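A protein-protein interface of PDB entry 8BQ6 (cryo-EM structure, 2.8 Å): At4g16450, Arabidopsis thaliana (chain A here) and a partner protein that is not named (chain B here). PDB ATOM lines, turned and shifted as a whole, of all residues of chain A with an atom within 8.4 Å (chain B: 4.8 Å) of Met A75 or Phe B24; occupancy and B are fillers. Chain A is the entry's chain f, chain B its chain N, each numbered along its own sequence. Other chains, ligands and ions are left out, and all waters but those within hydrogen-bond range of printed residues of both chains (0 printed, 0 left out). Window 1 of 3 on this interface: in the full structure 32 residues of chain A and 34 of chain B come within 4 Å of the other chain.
The backbone carbonyl oxygen (O) of Ser B61 lies within hydrogen-bond range of the side-chain hydroxyl (OG1) of Thr B65 (2.8 Å).
OG of Ser A44 lies within hydrogen-bond range of O of Ile A40.
The backbone carbonyl oxygen of Tyr A76 is in hydrogen-bond range of the side-chain amide nitrogen of Asn A80 (2.9 Å).
The backbone carbonyl oxygen of Leu B68 sits at hydrogen-bond distance from the side-chain amide nitrogen of Gln A79, at 3.2 Å.
Ile B64 touches Ser A44.
Ile A68 touches Phe B24 (O to CE1, 3.7 Å).
Ile A68 touches Ser B61 (CG2 to OG, 3.8 Å).
CE1 of Phe B24 touches CE of Met A71, 3.5 Å away.
Asn B27 touches Met A71 (CB to SD, 3.7 Å).
Met A71 touches Ala B28 (CE to N, 3.7 Å).
CA of Gly A72 touches CE1 of Phe B24 (3.6 Å).
Met A75 touches Phe B20.
SD of Met A75 touches CB of Phe B24 (3.9 Å).
Tyr A76 touches Leu B68 (N to CD2, 3.7 Å).
Of chain A, only Ile A68 (3.7 Å), Met A71 (3.5 Å), Gly A72 (3.6 Å) and Met A75 (3.9 Å) come within 4 Å of Phe B24.
Of the printed residues of chain A, Asn B27 touches Met A71 (3.7 Å).
Of the printed residues of chain A, Ser B61 touches Ile A68.
Of the printed residues of chain B, Ser A44 touches Ile B64 (3.8 Å).
Of the printed residues of chain B, Gly A72 touches Phe B24 (3.6 Å).
Of the printed residues of chain B, Met A71 touches Phe B24, Asn B27 and Ala B28.
Ala A82 touches none of the printed residues of chain B.
Of the 13 printed residues of chain B, 7 touch a printed residue of chain A.
Printed residues of chain B that touch a printed residue of chain A: Phe B20, Phe B24, Asn B27, Ala B28, Ser B61, Ile B64 and Leu B68.
Hydrophobic or aromatic side chains of chain B that line the printed part of chain A: Phe B20, Phe B24, Ala B28, Ile B64 and Leu B68.
Hydrophobic or aromatic side chains of chain A that line the printed part of chain B: Ile A68, Met A71, Met A75 and Tyr A76.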
ATOM      1  N   VAL A  25      -9.634  -3.217  27.449  1.00  0.00           N
ATOM      2  CA  VAL A  25      -8.483  -3.161  26.552  1.00  0.00           C
ATOM      3  C   VAL A  25      -8.301  -4.494  25.835  1.00  0.00           C
ATOM      4  O   VAL A  25      -7.986  -4.534  24.639  1.00  0.00           O
ATOM      5  CB  VAL A  25      -7.216  -2.751  27.325  1.00  0.00           C
ATOM      6  CG1 VAL A  25      -6.001  -2.758  26.414  1.00  0.00           C
ATOM      7  CG2 VAL A  25      -7.399  -1.383  27.940  1.00  0.00           C
ATOM      8  N   PHE A  29      -8.874  -5.606  21.320  1.00  0.00           N
ATOM      9  CA  PHE A  29      -7.837  -6.161  20.459  1.00  0.00           C
ATOM     10  C   PHE A  29      -8.321  -6.268  19.019  1.00  0.00           C
ATOM     11  O   PHE A  29      -9.385  -6.835  18.746  1.00  0.00           O
ATOM     12  CB  PHE A  29      -7.409  -7.535  20.965  1.00  0.00           C
ATOM     13  CG  PHE A  29      -6.478  -7.484  22.132  1.00  0.00           C
ATOM     14  CD1 PHE A  29      -6.011  -6.274  22.614  1.00  0.00           C
ATOM     15  CD2 PHE A  29      -6.068  -8.647  22.750  1.00  0.00           C
ATOM     16  CE1 PHE A  29      -5.159  -6.229  23.690  1.00  0.00           C
ATOM     17  CE2 PHE A  29      -5.216  -8.607  23.825  1.00  0.00           C
ATOM     18  CZ  PHE A  29      -4.760  -7.396  24.296  1.00  0.00           C
ATOM     19  N   PHE A  37       0.674 -10.294  18.204  1.00  0.00           N
ATOM     20  CA  PHE A  37       0.692 -11.346  19.211  1.00  0.00           C
ATOM     21  C   PHE A  37       1.174 -12.667  18.620  1.00  0.00           C
ATOM     22  O   PHE A  37       2.110 -13.297  19.137  1.00  0.00           O
ATOM     23  CB  PHE A  37      -0.719 -11.480  19.781  1.00  0.00           C
ATOM     24  CG  PHE A  37      -0.790 -12.184  21.087  1.00  0.00           C
ATOM     25  CD1 PHE A  37       0.331 -12.756  21.649  1.00  0.00           C
ATOM     26  CD2 PHE A  37      -1.988 -12.273  21.761  1.00  0.00           C
ATOM     27  CE1 PHE A  37       0.256 -13.407  22.846  1.00  0.00           C
ATOM     28  CE2 PHE A  37      -2.063 -12.918  22.961  1.00  0.00           C
ATOM     29  CZ  PHE A  37      -0.939 -13.489  23.503  1.00  0.00           C
ATOM     30  N   ILE A  40       4.962 -12.661  17.435  1.00  0.00           N
ATOM     31  CA  ILE A  40       5.922 -12.754  18.533  1.00  0.00           C
ATOM     32  C   ILE A  40       5.923 -14.159  19.119  1.00  0.00           C
ATOM     33  O   ILE A  40       6.986 -14.756  19.345  1.00  0.00           O
ATOM     34  CB  ILE A  40       5.623 -11.685  19.601  1.00  0.00           C
ATOM     35  CG1 ILE A  40       5.954 -10.300  19.053  1.00  0.00           C
ATOM     36  CG2 ILE A  40       6.434 -11.936  20.863  1.00  0.00           C
ATOM     37  CD1 ILE A  40       5.126  -9.201  19.659  1.00  0.00           C
ATOM     38  N   SER A  44       9.025 -16.892  18.977  1.00  0.00           N
ATOM     39  CA  SER A  44       9.593 -17.337  20.242  1.00  0.00           C
ATOM     40  C   SER A  44       9.580 -18.857  20.357  1.00  0.00           C
ATOM     41  O   SER A  44      10.556 -19.459  20.825  1.00  0.00           O
ATOM     42  CB  SER A  44       8.825 -16.694  21.385  1.00  0.00           C
ATOM     43  OG  SER A  44       9.093 -15.306  21.425  1.00  0.00           O
ATOM     44  N   GLY A  65      10.346 -21.023  25.384  1.00  0.00           N
ATOM     45  CA  GLY A  65      10.322 -19.931  24.430  1.00  0.00           C
ATOM     46  C   GLY A  65       8.913 -19.463  24.130  1.00  0.00           C
ATOM     47  O   GLY A  65       8.663 -18.264  23.998  1.00  0.00           O
ATOM     48  N   LEU A  67       6.335 -19.575  26.170  1.00  0.00           N
ATOM     49  CA  LEU A  67       5.842 -18.810  27.314  1.00  0.00           C
ATOM     50  C   LEU A  67       6.391 -17.390  27.297  1.00  0.00           C
ATOM     51  O   LEU A  67       5.657 -16.416  27.534  1.00  0.00           O
ATOM     52  CB  LEU A  67       6.234 -19.502  28.616  1.00  0.00           C
ATOM     53  CG  LEU A  67       5.409 -20.647  29.193  1.00  0.00           C
ATOM     54  CD1 LEU A  67       6.272 -21.343  30.218  1.00  0.00           C
ATOM     55  CD2 LEU A  67       4.117 -20.155  29.829  1.00  0.00           C
ATOM     56  N   ILE A  68       7.695 -17.255  27.036  1.00  0.00           N
ATOM     57  CA  ILE A  68       8.285 -15.921  26.946  1.00  0.00           C
ATOM     58  C   ILE A  68       7.600 -15.123  25.843  1.00  0.00           C
ATOM     59  O   ILE A  68       7.232 -13.954  26.033  1.00  0.00           O
ATOM     60  CB  ILE A  68       9.808 -16.021  26.732  1.00  0.00           C
ATOM     61  CG1 ILE A  68      10.496 -16.433  28.033  1.00  0.00           C
ATOM     62  CG2 ILE A  68      10.378 -14.700  26.255  1.00  0.00           C
ATOM     63  CD1 ILE A  68      11.922 -16.878  27.856  1.00  0.00           C
ATOM     64  N   GLY A  69       7.380 -15.757  24.690  1.00  0.00           N
ATOM     65  CA  GLY A  69       6.712 -15.084  23.591  1.00  0.00           C
ATOM     66  C   GLY A  69       5.260 -14.752  23.874  1.00  0.00           C
ATOM     67  O   GLY A  69       4.764 -13.716  23.439  1.00  0.00           O
ATOM     68  N   LEU A  70       4.554 -15.627  24.589  1.00  0.00           N
ATOM     69  CA  LEU A  70       3.162 -15.354  24.920  1.00  0.00           C
ATOM     70  C   LEU A  70       3.048 -14.139  25.821  1.00  0.00           C
ATOM     71  O   LEU A  70       2.236 -13.239  25.574  1.00  0.00           O
ATOM     72  CB  LEU A  70       2.530 -16.569  25.586  1.00  0.00           C
ATOM     73  CG  LEU A  70       1.855 -17.515  24.607  1.00  0.00           C
ATOM     74  CD1 LEU A  70       1.174 -18.615  25.377  1.00  0.00           C
ATOM     75  CD2 LEU A  70       0.859 -16.744  23.759  1.00  0.00           C
ATOM     76  N   MET A  71       3.875 -14.090  26.866  1.00  0.00           N
ATOM     77  CA  MET A  71       3.856 -12.935  27.753  1.00  0.00           C
ATOM     78  C   MET A  71       4.237 -11.659  27.003  1.00  0.00           C
ATOM     79  O   MET A  71       3.547 -10.636  27.106  1.00  0.00           O
ATOM     80  CB  MET A  71       4.777 -13.192  28.947  1.00  0.00           C
ATOM     81  CG  MET A  71       5.591 -12.006  29.412  1.00  0.00           C
ATOM     82  SD  MET A  71       6.580 -12.397  30.871  1.00  0.00           S
ATOM     83  CE  MET A  71       8.022 -13.155  30.127  1.00  0.00           C
ATOM     84  N   GLY A  72       5.305 -11.714  26.197  1.00  0.00           N
ATOM     85  CA  GLY A  72       5.745 -10.520  25.487  1.00  0.00           C
ATOM     86  C   GLY A  72       4.757 -10.042  24.437  1.00  0.00           C
ATOM     87  O   GLY A  72       4.529  -8.839  24.284  1.00  0.00           O
ATOM     88  N   GLY A  73       4.160 -10.977  23.694  1.00  0.00           N
ATOM     89  CA  GLY A  73       3.181 -10.609  22.686  1.00  0.00           C
ATOM     90  C   GLY A  73       1.889 -10.081  23.275  1.00  0.00           C
ATOM     91  O   GLY A  73       1.305  -9.129  22.750  1.00  0.00           O
ATOM     92  N   PHE A  74       1.414 -10.694  24.365  1.00  0.00           N
ATOM     93  CA  PHE A  74       0.237 -10.152  25.030  1.00  0.00           C
ATOM     94  C   PHE A  74       0.509  -8.760  25.571  1.00  0.00           C
ATOM     95  O   PHE A  74      -0.343  -7.871  25.469  1.00  0.00           O
ATOM     96  CB  PHE A  74      -0.220 -11.063  26.162  1.00  0.00           C
ATOM     97  CG  PHE A  74      -1.424 -10.545  26.893  1.00  0.00           C
ATOM     98  CD1 PHE A  74      -2.692 -10.740  26.380  1.00  0.00           C
ATOM     99  CD2 PHE A  74      -1.288  -9.844  28.080  1.00  0.00           C
ATOM    100  CE1 PHE A  74      -3.802 -10.260  27.044  1.00  0.00           C
ATOM    101  CE2 PHE A  74      -2.398  -9.361  28.747  1.00  0.00           C
ATOM    102  CZ  PHE A  74      -3.654  -9.571  28.228  1.00  0.00           C
ATOM    103  N   MET A  75       1.688  -8.552  26.162  1.00  0.00           N
ATOM    104  CA  MET A  75       2.015  -7.232  26.684  1.00  0.00           C
ATOM    105  C   MET A  75       2.073  -6.200  25.564  1.00  0.00           C
ATOM    106  O   MET A  75       1.568  -5.084  25.716  1.00  0.00           O
ATOM    107  CB  MET A  75       3.339  -7.296  27.447  1.00  0.00           C
ATOM    108  CG  MET A  75       3.173  -7.745  28.893  1.00  0.00           C
ATOM    109  SD  MET A  75       4.706  -7.835  29.833  1.00  0.00           S
ATOM    110  CE  MET A  75       4.980  -6.110  30.195  1.00  0.00           C
ATOM    111  N   TYR A  76       2.666  -6.566  24.424  1.00  0.00           N
ATOM    112  CA  TYR A  76       2.732  -5.661  23.279  1.00  0.00           C
ATOM    113  C   TYR A  76       1.346  -5.319  22.737  1.00  0.00           C
ATOM    114  O   TYR A  76       1.048  -4.148  22.450  1.00  0.00           O
ATOM    115  CB  TYR A  76       3.581  -6.300  22.186  1.00  0.00           C
ATOM    116  CG  TYR A  76       3.986  -5.347  21.102  1.00  0.00           C
ATOM    117  CD1 TYR A  76       4.541  -4.119  21.404  1.00  0.00           C
ATOM    118  CD2 TYR A  76       3.778  -5.664  19.771  1.00  0.00           C
ATOM    119  CE1 TYR A  76       4.902  -3.245  20.414  1.00  0.00           C
ATOM    120  CE2 TYR A  76       4.132  -4.795  18.774  1.00  0.00           C
ATOM    121  CZ  TYR A  76       4.695  -3.588  19.101  1.00  0.00           C
ATOM    122  OH  TYR A  76       5.053  -2.718  18.104  1.00  0.00           O
ATOM    123  N   ALA A  77       0.494  -6.332  22.570  1.00  0.00           N
ATOM    124  CA  ALA A  77      -0.860  -6.089  22.088  1.00  0.00           C
ATOM    125  C   ALA A  77      -1.644  -5.219  23.063  1.00  0.00           C
ATOM    126  O   ALA A  77      -2.379  -4.315  22.645  1.00  0.00           O
ATOM    127  CB  ALA A  77      -1.578  -7.416  21.857  1.00  0.00           C
ATOM    128  N   TYR A  78      -1.511  -5.486  24.366  1.00  0.00           N
ATOM    129  CA  TYR A  78      -2.171  -4.653  25.362  1.00  0.00           C
ATOM    130  C   TYR A  78      -1.678  -3.220  25.279  1.00  0.00           C
ATOM    131  O   TYR A  78      -2.469  -2.275  25.352  1.00  0.00           O
ATOM    132  CB  TYR A  78      -1.932  -5.209  26.769  1.00  0.00           C
ATOM    133  CG  TYR A  78      -2.684  -4.450  27.840  1.00  0.00           C
ATOM    134  CD1 TYR A  78      -2.243  -3.211  28.290  1.00  0.00           C
ATOM    135  CD2 TYR A  78      -3.849  -4.962  28.384  1.00  0.00           C
ATOM    136  CE1 TYR A  78      -2.936  -2.511  29.242  1.00  0.00           C
ATOM    137  CE2 TYR A  78      -4.548  -4.268  29.345  1.00  0.00           C
ATOM    138  CZ  TYR A  78      -4.087  -3.041  29.768  1.00  0.00           C
ATOM    139  OH  TYR A  78      -4.774  -2.339  30.727  1.00  0.00           O
ATOM    140  N   GLN A  79      -0.363  -3.047  25.164  1.00  0.00           N
ATOM    141  CA  GLN A  79       0.233  -1.730  25.018  1.00  0.00           C
ATOM    142  C   GLN A  79      -0.429  -0.961  23.887  1.00  0.00           C
ATOM    143  O   GLN A  79      -0.879   0.177  24.064  1.00  0.00           O
ATOM    144  CB  GLN A  79       1.724  -1.906  24.750  1.00  0.00           C
ATOM    145  CG  GLN A  79       2.601  -0.781  25.173  1.00  0.00           C
ATOM    146  CD  GLN A  79       4.046  -1.067  24.853  1.00  0.00           C
ATOM    147  OE1 GLN A  79       4.405  -1.291  23.699  1.00  0.00           O
ATOM    148  NE2 GLN A  79       4.885  -1.080  25.878  1.00  0.00           N
ATOM    149  N   ASN A  80      -0.528  -1.596  22.717  1.00  0.00           N
ATOM    150  CA  ASN A  80      -1.090  -0.912  21.555  1.00  0.00           C
ATOM    151  C   ASN A  80      -2.571  -0.601  21.747  1.00  0.00           C
ATOM    152  O   ASN A  80      -3.023   0.518  21.471  1.00  0.00           O
ATOM    153  CB  ASN A  80      -0.865  -1.749  20.302  1.00  0.00           C
ATOM    154  CG  ASN A  80       0.507  -1.547  19.721  1.00  0.00           C
ATOM    155  OD1 ASN A  80       0.705  -0.683  18.873  1.00  0.00           O
ATOM    156  ND2 ASN A  80       1.468  -2.340  20.172  1.00  0.00           N
ATOM    157  N   SER A  81      -3.342  -1.581  22.223  1.00  0.00           N
ATOM    158  CA  SER A  81      -4.777  -1.383  22.407  1.00  0.00           C
ATOM    159  C   SER A  81      -5.066  -0.268  23.409  1.00  0.00           C
ATOM    160  O   SER A  81      -5.906   0.609  23.164  1.00  0.00           O
ATOM    161  CB  SER A  81      -5.414  -2.695  22.862  1.00  0.00           C
ATOM    162  OG  SER A  81      -6.820  -2.591  22.944  1.00  0.00           O
ATOM    163  N   ALA A  82      -4.376  -0.288  24.552  1.00  0.00           N
ATOM    164  CA  ALA A  82      -4.605   0.725  25.572  1.00  0.00           C
ATOM    165  C   ALA A  82      -4.139   2.095  25.102  1.00  0.00           C
ATOM    166  O   ALA A  82      -4.781   3.109  25.396  1.00  0.00           O
ATOM    167  CB  ALA A  82      -3.907   0.332  26.872  1.00  0.00           C
ATOM    168  N   PHE B  20       6.310  -1.477  31.824  1.00  0.00           N
ATOM    169  CA  PHE B  20       6.131  -2.688  31.021  1.00  0.00           C
ATOM    170  C   PHE B  20       7.443  -3.314  30.556  1.00  0.00           C
ATOM    171  O   PHE B  20       7.602  -4.539  30.707  1.00  0.00           O
ATOM    172  CB  PHE B  20       5.223  -2.383  29.825  1.00  0.00           C
ATOM    173  CG  PHE B  20       3.828  -2.891  29.984  1.00  0.00           C
ATOM    174  CD1 PHE B  20       3.269  -3.036  31.238  1.00  0.00           C
ATOM    175  CD2 PHE B  20       3.079  -3.245  28.877  1.00  0.00           C
ATOM    176  CE1 PHE B  20       1.988  -3.510  31.385  1.00  0.00           C
ATOM    177  CE2 PHE B  20       1.797  -3.722  29.020  1.00  0.00           C
ATOM    178  CZ  PHE B  20       1.251  -3.853  30.276  1.00  0.00           C
ATOM    179  N   PRO B  21       8.398  -2.573  29.979  1.00  0.00           N
ATOM    180  CA  PRO B  21       9.662  -3.218  29.576  1.00  0.00           C
ATOM    181  C   PRO B  21      10.389  -3.906  30.722  1.00  0.00           C
ATOM    182  O   PRO B  21      10.858  -5.046  30.574  1.00  0.00           O
ATOM    183  CB  PRO B  21      10.473  -2.047  29.004  1.00  0.00           C
ATOM    184  CG  PRO B  21       9.462  -1.025  28.637  1.00  0.00           C
ATOM    185  CD  PRO B  21       8.412  -1.131  29.676  1.00  0.00           C
ATOM    186  N   GLU B  22      10.480  -3.239  31.875  1.00  0.00           N
ATOM    187  CA  GLU B  22      11.176  -3.820  33.019  1.00  0.00           C
ATOM    188  C   GLU B  22      10.437  -5.037  33.557  1.00  0.00           C
ATOM    189  O   GLU B  22      11.063  -6.052  33.893  1.00  0.00           O
ATOM    190  CB  GLU B  22      11.345  -2.770  34.115  1.00  0.00           C
ATOM    191  CG  GLU B  22      12.478  -1.792  33.869  1.00  0.00           C
ATOM    192  CD  GLU B  22      12.038  -0.573  33.078  1.00  0.00           C
ATOM    193  OE1 GLU B  22      12.906   0.092  32.476  1.00  0.00           O
ATOM    194  OE2 GLU B  22      10.823  -0.283  33.049  1.00  0.00           O
ATOM    195  N   ILE B  23       9.109  -4.953  33.657  1.00  0.00           N
ATOM    196  CA  ILE B  23       8.333  -6.099  34.115  1.00  0.00           C
ATOM    197  C   ILE B  23       8.603  -7.294  33.215  1.00  0.00           C
ATOM    198  O   ILE B  23       8.860  -8.411  33.686  1.00  0.00           O
ATOM    199  CB  ILE B  23       6.832  -5.761  34.147  1.00  0.00           C
ATOM    200  CG1 ILE B  23       6.503  -4.847  35.318  1.00  0.00           C
ATOM    201  CG2 ILE B  23       6.013  -7.029  34.300  1.00  0.00           C
ATOM    202  CD1 ILE B  23       5.077  -4.362  35.290  1.00  0.00           C
ATOM    203  N   PHE B  24       8.573  -7.065  31.898  1.00  0.00           N
ATOM    204  CA  PHE B  24       8.787  -8.170  30.976  1.00  0.00           C
ATOM    205  C   PHE B  24      10.177  -8.768  31.135  1.00  0.00           C
ATOM    206  O   PHE B  24      10.330  -9.994  31.183  1.00  0.00           O
ATOM    207  CB  PHE B  24       8.578  -7.745  29.525  1.00  0.00           C
ATOM    208  CG  PHE B  24       9.040  -8.787  28.563  1.00  0.00           C
ATOM    209  CD1 PHE B  24       8.269  -9.909  28.332  1.00  0.00           C
ATOM    210  CD2 PHE B  24      10.275  -8.690  27.948  1.00  0.00           C
ATOM    211  CE1 PHE B  24       8.703 -10.897  27.485  1.00  0.00           C
ATOM    212  CE2 PHE B  24      10.711  -9.677  27.102  1.00  0.00           C
ATOM    213  CZ  PHE B  24       9.921 -10.781  26.868  1.00  0.00           C
ATOM    214  N   ILE B  25      11.213  -7.926  31.192  1.00  0.00           N
ATOM    215  CA  ILE B  25      12.563  -8.483  31.230  1.00  0.00           C
ATOM    216  C   ILE B  25      12.808  -9.226  32.542  1.00  0.00           C
ATOM    217  O   ILE B  25      13.456 -10.280  32.557  1.00  0.00           O
ATOM    218  CB  ILE B  25      13.631  -7.404  30.958  1.00  0.00           C
ATOM    219  CG1 ILE B  25      15.000  -8.072  30.782  1.00  0.00           C
ATOM    220  CG2 ILE B  25      13.657  -6.338  32.041  1.00  0.00           C
ATOM    221  CD1 ILE B  25      15.977  -7.296  29.927  1.00  0.00           C
ATOM    222  N   ILE B  26      12.266  -8.725  33.653  1.00  0.00           N
ATOM    223  CA  ILE B  26      12.462  -9.400  34.935  1.00  0.00           C
ATOM    224  C   ILE B  26      11.752 -10.751  34.944  1.00  0.00           C
ATOM    225  O   ILE B  26      12.311 -11.768  35.385  1.00  0.00           O
ATOM    226  CB  ILE B  26      11.992  -8.500  36.091  1.00  0.00           C
ATOM    227  CG1 ILE B  26      12.932  -7.308  36.232  1.00  0.00           C
ATOM    228  CG2 ILE B  26      11.976  -9.259  37.390  1.00  0.00           C
ATOM    229  CD1 ILE B  26      12.415  -6.232  37.138  1.00  0.00           C
ATOM    230  N   ASN B  27      10.509 -10.788  34.455  1.00  0.00           N
ATOM    231  CA  ASN B  27       9.774 -12.048  34.439  1.00  0.00           C
ATOM    232  C   ASN B  27      10.427 -13.059  33.505  1.00  0.00           C
ATOM    233  O   ASN B  27      10.482 -14.258  33.810  1.00  0.00           O
ATOM    234  CB  ASN B  27       8.326 -11.800  34.035  1.00  0.00           C
ATOM    235  CG  ASN B  27       7.433 -11.534  35.223  1.00  0.00           C
ATOM    236  OD1 ASN B  27       7.651 -12.066  36.311  1.00  0.00           O
ATOM    237  ND2 ASN B  27       6.429 -10.694  35.027  1.00  0.00           N
ATOM    238  N   ALA B  28      10.923 -12.597  32.356  1.00  0.00           N
ATOM    239  CA  ALA B  28      11.622 -13.494  31.445  1.00  0.00           C
ATOM    240  C   ALA B  28      12.898 -14.032  32.080  1.00  0.00           C
ATOM    241  O   ALA B  28      13.253 -15.201  31.883  1.00  0.00           O
ATOM    242  CB  ALA B  28      11.927 -12.770  30.137  1.00  0.00           C
ATOM    243  N   SER B  61      14.694 -12.447  24.639  1.00  0.00           N
ATOM    244  CA  SER B  61      14.037 -11.642  25.669  1.00  0.00           C
ATOM    245  C   SER B  61      14.463 -10.180  25.594  1.00  0.00           C
ATOM    246  O   SER B  61      13.637  -9.274  25.756  1.00  0.00           O
ATOM    247  CB  SER B  61      14.336 -12.205  27.059  1.00  0.00           C
ATOM    248  OG  SER B  61      13.931 -13.556  27.169  1.00  0.00           O
ATOM    249  N   ILE B  64      12.730  -8.521  22.639  1.00  0.00           N
ATOM    250  CA  ILE B  64      11.321  -8.232  22.915  1.00  0.00           C
ATOM    251  C   ILE B  64      11.191  -7.055  23.878  1.00  0.00           C
ATOM    252  O   ILE B  64      10.275  -6.230  23.755  1.00  0.00           O
ATOM    253  CB  ILE B  64      10.599  -9.477  23.457  1.00  0.00           C
ATOM    254  CG1 ILE B  64      10.480 -10.540  22.371  1.00  0.00           C
ATOM    255  CG2 ILE B  64       9.208  -9.117  23.941  1.00  0.00           C
ATOM    256  CD1 ILE B  64       9.945 -11.849  22.878  1.00  0.00           C
ATOM    257  N   THR B  65      12.086  -6.971  24.866  1.00  0.00           N
ATOM    258  CA  THR B  65      12.113  -5.807  25.744  1.00  0.00           C
ATOM    259  C   THR B  65      12.356  -4.533  24.950  1.00  0.00           C
ATOM    260  O   THR B  65      11.707  -3.507  25.186  1.00  0.00           O
ATOM    261  CB  THR B  65      13.201  -5.974  26.803  1.00  0.00           C
ATOM    262  OG1 THR B  65      13.022  -7.216  27.492  1.00  0.00           O
ATOM    263  CG2 THR B  65      13.158  -4.833  27.796  1.00  0.00           C
ATOM    264  N   LEU B  68       9.199  -3.586  23.142  1.00  0.00           N
ATOM    265  CA  LEU B  68       8.231  -2.997  24.064  1.00  0.00           C
ATOM    266  C   LEU B  68       8.606  -1.567  24.424  1.00  0.00           C
ATOM    267  O   LEU B  68       7.736  -0.696  24.537  1.00  0.00           O
ATOM    268  CB  LEU B  68       8.131  -3.845  25.329  1.00  0.00           C
ATOM    269  CG  LEU B  68       7.263  -5.099  25.301  1.00  0.00           C
ATOM    270  CD1 LEU B  68       7.474  -5.872  26.580  1.00  0.00           C
ATOM    271  CD2 LEU B  68       5.803  -4.741  25.126  1.00  0.00           C
